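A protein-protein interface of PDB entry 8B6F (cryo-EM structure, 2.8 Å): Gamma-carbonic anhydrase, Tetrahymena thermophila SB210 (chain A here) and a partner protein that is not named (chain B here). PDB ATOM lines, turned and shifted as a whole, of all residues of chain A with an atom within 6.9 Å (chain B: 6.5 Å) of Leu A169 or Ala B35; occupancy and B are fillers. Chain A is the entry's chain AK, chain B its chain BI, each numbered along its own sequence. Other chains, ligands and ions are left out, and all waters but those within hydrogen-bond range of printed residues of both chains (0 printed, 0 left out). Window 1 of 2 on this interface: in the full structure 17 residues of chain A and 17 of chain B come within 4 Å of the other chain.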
ATOM      1  N   GLY A 149       7.418 -18.895  -4.648  1.00  0.00           N
ATOM      2  CA  GLY A 149       7.235 -20.093  -3.862  1.00  0.00           C
ATOM      3  C   GLY A 149       8.024 -21.297  -4.328  1.00  0.00           C
ATOM      4  O   GLY A 149       8.020 -22.322  -3.636  1.00  0.00           O
ATOM      5  N   ALA A 150       8.699 -21.209  -5.468  1.00  0.00           N
ATOM      6  CA  ALA A 150       9.470 -22.336  -5.969  1.00  0.00           C
ATOM      7  C   ALA A 150      10.678 -22.600  -5.080  1.00  0.00           C
ATOM      8  O   ALA A 150      11.272 -21.683  -4.508  1.00  0.00           O
ATOM      9  CB  ALA A 150       9.924 -22.074  -7.403  1.00  0.00           C
ATOM     10  N   ARG A 151      11.042 -23.875  -4.969  1.00  0.00           N
ATOM     11  CA  ARG A 151      12.169 -24.308  -4.146  1.00  0.00           C
ATOM     12  C   ARG A 151      13.042 -25.233  -4.986  1.00  0.00           C
ATOM     13  O   ARG A 151      12.688 -26.392  -5.214  1.00  0.00           O
ATOM     14  CB  ARG A 151      11.685 -25.002  -2.878  1.00  0.00           C
ATOM     15  CG  ARG A 151      12.788 -25.293  -1.875  1.00  0.00           C
ATOM     16  CD  ARG A 151      12.211 -25.780  -0.558  1.00  0.00           C
ATOM     17  NE  ARG A 151      13.198 -25.753   0.515  1.00  0.00           N
ATOM     18  CZ  ARG A 151      14.013 -26.753   0.817  1.00  0.00           C
ATOM     19  NH1 ARG A 151      13.995 -27.890   0.142  1.00  0.00           N
ATOM     20  NH2 ARG A 151      14.867 -26.610   1.825  1.00  0.00           N
ATOM     21  N   ILE A 152      14.178 -24.720  -5.445  1.00  0.00           N
ATOM     22  CA  ILE A 152      15.140 -25.496  -6.217  1.00  0.00           C
ATOM     23  C   ILE A 152      16.220 -25.972  -5.256  1.00  0.00           C
ATOM     24  O   ILE A 152      16.861 -25.157  -4.582  1.00  0.00           O
ATOM     25  CB  ILE A 152      15.747 -24.668  -7.360  1.00  0.00           C
ATOM     26  CG1 ILE A 152      14.666 -23.851  -8.079  1.00  0.00           C
ATOM     27  CG2 ILE A 152      16.477 -25.575  -8.339  1.00  0.00           C
ATOM     28  CD1 ILE A 152      13.594 -24.675  -8.736  1.00  0.00           C
ATOM     29  N   GLU A 153      16.427 -27.284  -5.188  1.00  0.00           N
ATOM     30  CA  GLU A 153      17.355 -27.850  -4.225  1.00  0.00           C
ATOM     31  C   GLU A 153      18.775 -27.879  -4.791  1.00  0.00           C
ATOM     32  O   GLU A 153      19.029 -27.509  -5.938  1.00  0.00           O
ATOM     33  CB  GLU A 153      16.894 -29.243  -3.806  1.00  0.00           C
ATOM     34  CG  GLU A 153      15.595 -29.238  -3.021  1.00  0.00           C
ATOM     35  CD  GLU A 153      15.205 -30.619  -2.537  1.00  0.00           C
ATOM     36  OE1 GLU A 153      15.793 -31.608  -3.021  1.00  0.00           O
ATOM     37  OE2 GLU A 153      14.316 -30.714  -1.665  1.00  0.00           O
ATOM     38  N   VAL A 164       9.349 -22.561 -13.952  1.00  0.00           N
ATOM     39  CA  VAL A 164       9.079 -23.289 -12.715  1.00  0.00           C
ATOM     40  C   VAL A 164       7.817 -22.690 -12.096  1.00  0.00           C
ATOM     41  O   VAL A 164       7.861 -21.547 -11.614  1.00  0.00           O
ATOM     42  CB  VAL A 164      10.266 -23.207 -11.746  1.00  0.00           C
ATOM     43  CG1 VAL A 164       9.918 -23.836 -10.401  1.00  0.00           C
ATOM     44  CG2 VAL A 164      11.486 -23.883 -12.345  1.00  0.00           C
ATOM     45  N   PRO A 165       6.694 -23.407 -12.077  1.00  0.00           N
ATOM     46  CA  PRO A 165       5.446 -22.825 -11.570  1.00  0.00           C
ATOM     47  C   PRO A 165       5.556 -22.478 -10.097  1.00  0.00           C
ATOM     48  O   PRO A 165       6.475 -22.942  -9.406  1.00  0.00           O
ATOM     49  CB  PRO A 165       4.413 -23.937 -11.804  1.00  0.00           C
ATOM     50  CG  PRO A 165       4.990 -24.776 -12.874  1.00  0.00           C
ATOM     51  CD  PRO A 165       6.471 -24.738 -12.669  1.00  0.00           C
ATOM     52  N   PRO A 166       4.642 -21.657  -9.581  1.00  0.00           N
ATOM     53  CA  PRO A 166       4.723 -21.264  -8.170  1.00  0.00           C
ATOM     54  C   PRO A 166       4.602 -22.464  -7.245  1.00  0.00           C
ATOM     55  O   PRO A 166       3.842 -23.399  -7.504  1.00  0.00           O
ATOM     56  CB  PRO A 166       3.539 -20.306  -7.998  1.00  0.00           C
ATOM     57  CG  PRO A 166       3.120 -19.927  -9.376  1.00  0.00           C
ATOM     58  CD  PRO A 166       3.443 -21.103 -10.231  1.00  0.00           C
ATOM     59  N   GLY A 167       5.357 -22.424  -6.153  1.00  0.00           N
ATOM     60  CA  GLY A 167       5.247 -23.460  -5.137  1.00  0.00           C
ATOM     61  C   GLY A 167       5.565 -24.850  -5.637  1.00  0.00           C
ATOM     62  O   GLY A 167       4.896 -25.814  -5.246  1.00  0.00           O
ATOM     63  N   ARG A 168       6.575 -24.977  -6.493  1.00  0.00           N
ATOM     64  CA  ARG A 168       7.019 -26.263  -7.010  1.00  0.00           C
ATOM     65  C   ARG A 168       8.413 -26.568  -6.486  1.00  0.00           C
ATOM     66  O   ARG A 168       9.260 -25.674  -6.387  1.00  0.00           O
ATOM     67  CB  ARG A 168       7.025 -26.274  -8.541  1.00  0.00           C
ATOM     68  CG  ARG A 168       5.644 -26.280  -9.169  1.00  0.00           C
ATOM     69  CD  ARG A 168       4.903 -27.568  -8.861  1.00  0.00           C
ATOM     70  NE  ARG A 168       3.613 -27.630  -9.536  1.00  0.00           N
ATOM     71  CZ  ARG A 168       2.503 -27.057  -9.088  1.00  0.00           C
ATOM     72  NH1 ARG A 168       2.494 -26.347  -7.971  1.00  0.00           N
ATOM     73  NH2 ARG A 168       1.376 -27.200  -9.777  1.00  0.00           N
ATOM     74  N   LEU A 169       8.647 -27.834  -6.156  1.00  0.00           N
ATOM     75  CA  LEU A 169       9.898 -28.284  -5.563  1.00  0.00           C
ATOM     76  C   LEU A 169      10.691 -29.056  -6.607  1.00  0.00           C
ATOM     77  O   LEU A 169      10.229 -30.085  -7.110  1.00  0.00           O
ATOM     78  CB  LEU A 169       9.633 -29.149  -4.329  1.00  0.00           C
ATOM     79  CG  LEU A 169      10.801 -29.347  -3.357  1.00  0.00           C
ATOM     80  CD1 LEU A 169      10.299 -29.903  -2.044  1.00  0.00           C
ATOM     81  CD2 LEU A 169      11.875 -30.259  -3.926  1.00  0.00           C
ATOM     82  N   ILE A 170      11.882 -28.557  -6.926  1.00  0.00           N
ATOM     83  CA  ILE A 170      12.798 -29.219  -7.850  1.00  0.00           C
ATOM     84  C   ILE A 170      13.829 -29.974  -7.013  1.00  0.00           C
ATOM     85  O   ILE A 170      14.613 -29.333  -6.294  1.00  0.00           O
ATOM     86  CB  ILE A 170      13.470 -28.208  -8.790  1.00  0.00           C
ATOM     87  CG1 ILE A 170      12.425 -27.500  -9.663  1.00  0.00           C
ATOM     88  CG2 ILE A 170      14.517 -28.887  -9.653  1.00  0.00           C
ATOM     89  CD1 ILE A 170      11.563 -28.417 -10.506  1.00  0.00           C
ATOM     90  N   PRO A 171      13.869 -31.306  -7.066  1.00  0.00           N
ATOM     91  CA  PRO A 171      14.783 -32.050  -6.194  1.00  0.00           C
ATOM     92  C   PRO A 171      16.243 -31.775  -6.516  1.00  0.00           C
ATOM     93  O   PRO A 171      16.604 -31.322  -7.604  1.00  0.00           O
ATOM     94  CB  PRO A 171      14.429 -33.517  -6.470  1.00  0.00           C
ATOM     95  CG  PRO A 171      13.073 -33.486  -7.053  1.00  0.00           C
ATOM     96  CD  PRO A 171      12.983 -32.211  -7.818  1.00  0.00           C
ATOM     97  N   ALA A 172      17.089 -32.063  -5.532  1.00  0.00           N
ATOM     98  CA  ALA A 172      18.520 -31.830  -5.669  1.00  0.00           C
ATOM     99  C   ALA A 172      19.122 -32.731  -6.740  1.00  0.00           C
ATOM    100  O   ALA A 172      18.763 -33.903  -6.866  1.00  0.00           O
ATOM    101  CB  ALA A 172      19.219 -32.073  -4.333  1.00  0.00           C
ATOM    102  N   TRP A 176      15.618 -30.469 -15.245  1.00  0.00           N
ATOM    103  CA  TRP A 176      14.244 -30.167 -15.618  1.00  0.00           C
ATOM    104  C   TRP A 176      14.240 -29.218 -16.805  1.00  0.00           C
ATOM    105  O   TRP A 176      15.095 -28.334 -16.905  1.00  0.00           O
ATOM    106  CB  TRP A 176      13.475 -29.553 -14.449  1.00  0.00           C
ATOM    107  CG  TRP A 176      13.324 -30.479 -13.288  1.00  0.00           C
ATOM    108  CD1 TRP A 176      14.300 -30.870 -12.425  1.00  0.00           C
ATOM    109  CD2 TRP A 176      12.120 -31.123 -12.852  1.00  0.00           C
ATOM    110  NE1 TRP A 176      13.782 -31.719 -11.482  1.00  0.00           N
ATOM    111  CE2 TRP A 176      12.445 -31.891 -11.721  1.00  0.00           C
ATOM    112  CE3 TRP A 176      10.800 -31.126 -13.311  1.00  0.00           C
ATOM    113  CZ2 TRP A 176      11.505 -32.656 -11.041  1.00  0.00           C
ATOM    114  CZ3 TRP A 176       9.864 -31.887 -12.635  1.00  0.00           C
ATOM    115  CH2 TRP A 176      10.222 -32.642 -11.511  1.00  0.00           C
ATOM    116  N   CYS A 181       8.038 -26.944 -16.394  1.00  0.00           N
ATOM    117  CA  CYS A 181       9.230 -27.775 -16.320  1.00  0.00           C
ATOM    118  C   CYS A 181       8.856 -29.222 -16.025  1.00  0.00           C
ATOM    119  O   CYS A 181       7.959 -29.500 -15.224  1.00  0.00           O
ATOM    120  CB  CYS A 181      10.180 -27.244 -15.247  1.00  0.00           C
ATOM    121  SG  CYS A 181       9.473 -27.212 -13.588  1.00  0.00           S
ATOM    122  N   THR A 182       9.552 -30.147 -16.683  1.00  0.00           N
ATOM    123  CA  THR A 182       9.346 -31.575 -16.497  1.00  0.00           C
ATOM    124  C   THR A 182      10.691 -32.255 -16.294  1.00  0.00           C
ATOM    125  O   THR A 182      11.719 -31.797 -16.793  1.00  0.00           O
ATOM    126  CB  THR A 182       8.624 -32.207 -17.696  1.00  0.00           C
ATOM    127  OG1 THR A 182       9.353 -31.932 -18.899  1.00  0.00           O
ATOM    128  CG2 THR A 182       7.212 -31.662 -17.822  1.00  0.00           C
ATOM    129  N   PHE A 183      10.665 -33.360 -15.555  1.00  0.00           N
ATOM    130  CA  PHE A 183      11.884 -34.081 -15.225  1.00  0.00           C
ATOM    131  C   PHE A 183      12.500 -34.700 -16.474  1.00  0.00           C
ATOM    132  O   PHE A 183      11.799 -35.113 -17.401  1.00  0.00           O
ATOM    133  CB  PHE A 183      11.573 -35.164 -14.192  1.00  0.00           C
ATOM    134  CG  PHE A 183      12.766 -35.954 -13.750  1.00  0.00           C
ATOM    135  CD1 PHE A 183      13.673 -35.417 -12.854  1.00  0.00           C
ATOM    136  CD2 PHE A 183      12.964 -37.246 -14.205  1.00  0.00           C
ATOM    137  CE1 PHE A 183      14.765 -36.146 -12.434  1.00  0.00           C
ATOM    138  CE2 PHE A 183      14.053 -37.981 -13.790  1.00  0.00           C
ATOM    139  CZ  PHE A 183      14.956 -37.430 -12.904  1.00  0.00           C
ATOM    140  N   HIS B  29      10.504 -39.529  -9.508  1.00  0.00           N
ATOM    141  CA  HIS B  29      10.126 -38.878 -10.751  1.00  0.00           C
ATOM    142  C   HIS B  29      10.629 -39.679 -11.942  1.00  0.00           C
ATOM    143  O   HIS B  29      11.722 -40.251 -11.905  1.00  0.00           O
ATOM    144  CB  HIS B  29      10.687 -37.456 -10.812  1.00  0.00           C
ATOM    145  CG  HIS B  29       9.919 -36.471  -9.990  1.00  0.00           C
ATOM    146  ND1 HIS B  29       8.638 -36.075 -10.313  1.00  0.00           N
ATOM    147  CD2 HIS B  29      10.248 -35.797  -8.865  1.00  0.00           C
ATOM    148  CE1 HIS B  29       8.212 -35.202  -9.419  1.00  0.00           C
ATOM    149  NE2 HIS B  29       9.170 -35.015  -8.529  1.00  0.00           N
ATOM    150  N   ASP B  33       7.633 -36.049 -15.883  1.00  0.00           N
ATOM    151  CA  ASP B  33       6.742 -35.814 -14.758  1.00  0.00           C
ATOM    152  C   ASP B  33       6.829 -34.365 -14.288  1.00  0.00           C
ATOM    153  O   ASP B  33       7.830 -33.676 -14.491  1.00  0.00           O
ATOM    154  CB  ASP B  33       7.076 -36.751 -13.596  1.00  0.00           C
ATOM    155  CG  ASP B  33       6.717 -38.191 -13.889  1.00  0.00           C
ATOM    156  OD1 ASP B  33       5.763 -38.424 -14.657  1.00  0.00           O
ATOM    157  OD2 ASP B  33       7.390 -39.093 -13.347  1.00  0.00           O
ATOM    158  N   GLN B  34       5.755 -33.912 -13.651  1.00  0.00           N
ATOM    159  CA  GLN B  34       5.687 -32.574 -13.088  1.00  0.00           C
ATOM    160  C   GLN B  34       6.230 -32.571 -11.664  1.00  0.00           C
ATOM    161  O   GLN B  34       6.152 -33.571 -10.947  1.00  0.00           O
ATOM    162  CB  GLN B  34       4.247 -32.057 -13.090  1.00  0.00           C
ATOM    163  CG  GLN B  34       3.624 -31.932 -14.475  1.00  0.00           C
ATOM    164  CD  GLN B  34       4.387 -30.989 -15.395  1.00  0.00           C
ATOM    165  OE1 GLN B  34       4.391 -31.170 -16.613  1.00  0.00           O
ATOM    166  NE2 GLN B  34       5.024 -29.972 -14.821  1.00  0.00           N
ATOM    167  N   ALA B  35       6.776 -31.429 -11.262  1.00  0.00           N
ATOM    168  CA  ALA B  35       7.361 -31.302  -9.936  1.00  0.00           C
ATOM    169  C   ALA B  35       6.279 -31.307  -8.864  1.00  0.00           C
ATOM    170  O   ALA B  35       5.149 -30.863  -9.084  1.00  0.00           O
ATOM    171  CB  ALA B  35       8.185 -30.020  -9.839  1.00  0.00           C
ATOM    172  N   ASP B  36       6.636 -31.820  -7.691  1.00  0.00           N
ATOM    173  CA  ASP B  36       5.711 -31.868  -6.569  1.00  0.00           C
ATOM    174  C   ASP B  36       5.609 -30.504  -5.897  1.00  0.00           C
ATOM    175  O   ASP B  36       6.541 -29.697  -5.928  1.00  0.00           O
ATOM    176  CB  ASP B  36       6.155 -32.912  -5.546  1.00  0.00           C
ATOM    177  CG  ASP B  36       6.066 -34.326  -6.081  1.00  0.00           C
ATOM    178  OD1 ASP B  36       6.958 -34.727  -6.855  1.00  0.00           O
ATOM    179  OD2 ASP B  36       5.103 -35.039  -5.728  1.00  0.00           O
ATOM    180  N   ARG B  37       4.459 -30.259  -5.281  1.00  0.00           N
ATOM    181  CA  ARG B  37       4.230 -28.999  -4.591  1.00  0.00           C
ATOM    182  C   ARG B  37       5.018 -28.944  -3.291  1.00  0.00           C
ATOM    183  O   ARG B  37       5.165 -29.948  -2.589  1.00  0.00           O
ATOM    184  CB  ARG B  37       2.741 -28.821  -4.305  1.00  0.00           C
ATOM    185  CG  ARG B  37       1.892 -28.644  -5.549  1.00  0.00           C
ATOM    186  CD  ARG B  37       0.448 -29.024  -5.284  1.00  0.00           C
ATOM    187  NE  ARG B  37      -0.044 -28.455  -4.037  1.00  0.00           N
ATOM    188  CZ  ARG B  37      -1.244 -28.692  -3.526  1.00  0.00           C
ATOM    189  NH1 ARG B  37      -2.112 -29.477  -4.140  1.00  0.00           N
ATOM    190  NH2 ARG B  37      -1.579 -28.129  -2.370  1.00  0.00           N
ATOM    191  N   VAL B  38       5.526 -27.754  -2.969  1.00  0.00           N
ATOM    192  CA  VAL B  38       6.208 -27.561  -1.696  1.00  0.00           C
ATOM    193  C   VAL B  38       5.228 -27.709  -0.540  1.00  0.00           C
ATOM    194  O   VAL B  38       5.617 -28.106   0.563  1.00  0.00           O
ATOM    195  CB  VAL B  38       6.910 -26.189  -1.669  1.00  0.00           C
ATOM    196  CG1 VAL B  38       7.565 -25.944  -0.320  1.00  0.00           C
ATOM    197  CG2 VAL B  38       7.944 -26.097  -2.775  1.00  0.00           C
ATOM    198  N   LYS B  41       5.198 -31.066   0.925  1.00  0.00           N
ATOM    199  CA  LYS B  41       6.468 -31.461   1.517  1.00  0.00           C
ATOM    200  C   LYS B  41       6.822 -30.711   2.793  1.00  0.00           C
ATOM    201  O   LYS B  41       7.673 -31.191   3.549  1.00  0.00           O
ATOM    202  CB  LYS B  41       7.606 -31.262   0.504  1.00  0.00           C
ATOM    203  CG  LYS B  41       7.469 -32.098  -0.759  1.00  0.00           C
ATOM    204  CD  LYS B  41       7.553 -33.585  -0.459  1.00  0.00           C
ATOM    205  CE  LYS B  41       7.631 -34.402  -1.738  1.00  0.00           C
ATOM    206  NZ  LYS B  41       6.454 -34.180  -2.620  1.00  0.00           N
ATOM    207  N   PHE B  60      11.661 -28.360   6.671  1.00  0.00           N
ATOM    208  CA  PHE B  60      11.890 -29.377   5.658  1.00  0.00           C
ATOM    209  C   PHE B  60      12.806 -30.447   6.229  1.00  0.00           C
ATOM    210  O   PHE B  60      13.563 -30.209   7.171  1.00  0.00           O
ATOM    211  CB  PHE B  60      12.510 -28.780   4.387  1.00  0.00           C
ATOM    212  CG  PHE B  60      11.606 -27.827   3.661  1.00  0.00           C
ATOM    213  CD1 PHE B  60      11.560 -26.491   4.020  1.00  0.00           C
ATOM    214  CD2 PHE B  60      10.807 -28.266   2.620  1.00  0.00           C
ATOM    215  CE1 PHE B  60      10.731 -25.610   3.356  1.00  0.00           C
ATOM    216  CE2 PHE B  60       9.975 -27.389   1.952  1.00  0.00           C
ATOM    217  CZ  PHE B  60       9.940 -26.058   2.319  1.00  0.00           C
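The backbone carbonyl oxygen (O) of Gly A167 lies within hydrogen-bond range of the backbone NH (N) of Val B38. The backbone carbonyl oxygen (O) of Asp B36 is in hydrogen-bond range of the backbone NH (N) of Leu A169 (2.8 Å). The side-chain amide nitrogen of Gln B34 is in hydrogen-bond range of the backbone carbonyl oxygen of Cys A181 (3.0 Å). O of Asp B33 lies within hydrogen-bond range of N of Phe A183, 3.0 Å away.
The guanidinium group (NH1) of Arg A151 lies within salt-bridge range of the side-chain carboxylate (OE2) of Glu A153 (3.4 Å). The backbone carbonyl oxygen (O) of Arg A168 lies within hydrogen-bond range of the backbone NH (N) of Arg A151, at 2.9 Å. The backbone carbonyl oxygen (O) of Arg A151 is in hydrogen-bond range of the backbone NH (N) of Ile A170 (2.9 Å). The backbone carbonyl oxygen (O) of Ile A170 sits at hydrogen-bond distance from the backbone NH (N) of Glu A153 (3.0 Å). NH1 of Arg A168 lies within hydrogen-bond range of O of Pro A166, 3.3 Å away. OD2 of Asp B36 is in salt-bridge range of NZ of Lys B41 (3.5 Å).
Among the printed residues, pairs that only touch across the chains: Thr A182 with Gln B34, Thr A182 with Asp B33, Trp A176 with Asp B33, Arg A168 with Ala B35, Gly A167 with Arg B37, Arg A168 with Arg B37, Leu A169 with Ala B35, Trp A176 with Ala B35, Arg A168 with Asp B36, Arg A151 with Phe B60, Phe A183 with His B29, Arg A168 with Val B38, Ile A170 with Ala B35, Leu A169 with Lys B41, Leu A169 with Val B38, Trp A176 with Gln B34, Trp A176 with His B29, Gly A149 with Val B38 and Arg A151 with Val B38.
Ile A152 touches none of the printed residues of chain B. Of the printed residues of chain B, Leu A169 touches Ala B35, Asp B36, Val B38 and Lys B41. Of the printed residues of chain B, Phe A183 touches His B29 (3.8 Å) and Asp B33 (3.0 Å). Of chain A, only Arg A168, Leu A169, Ile A170 and Trp A176 come within 4 Å of Ala B35. Of the printed residues of chain A, Asp B36 touches Arg A168 (3.6 Å) and Leu A169 (2.8 Å). Of the printed residues of chain A, Arg B37 touches Gly A167 (3.3 Å) and Arg A168 (3.4 Å). Of the printed residues of chain A, Val B38 touches Gly A149 (3.9 Å), Arg A151 (3.9 Å), Gly A167 (3.1 Å), Arg A168 (3.8 Å) and Leu A169 (3.8 Å). The nearest residue of chain A that does not touch Ala B35 is Cys A181 (4.6 Å). The nearest printed residue of chain A that does not touch Lys B41 is Glu A153 (7.0 Å).
Printed residues of chain B that touch a printed residue of chain A: His B29, Asp B33, Gln B34, Ala B35, Asp B36, Arg B37, Val B38, Lys B41 and Phe B60. Hydrophobic or aromatic side chains of chain B that line the printed part of chain A: His B29, Ala B35, Val B38 and Phe B60. Along chain A the printed residues that touch a printed residue of chain B span positions 149 to 183. Among the printed residues, 23 pairs touch across the chains. Among the printed residues, no Asp or Glu carboxylate lies within 4 Å of a Lys or Arg side-chain nitrogen of the other chain.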
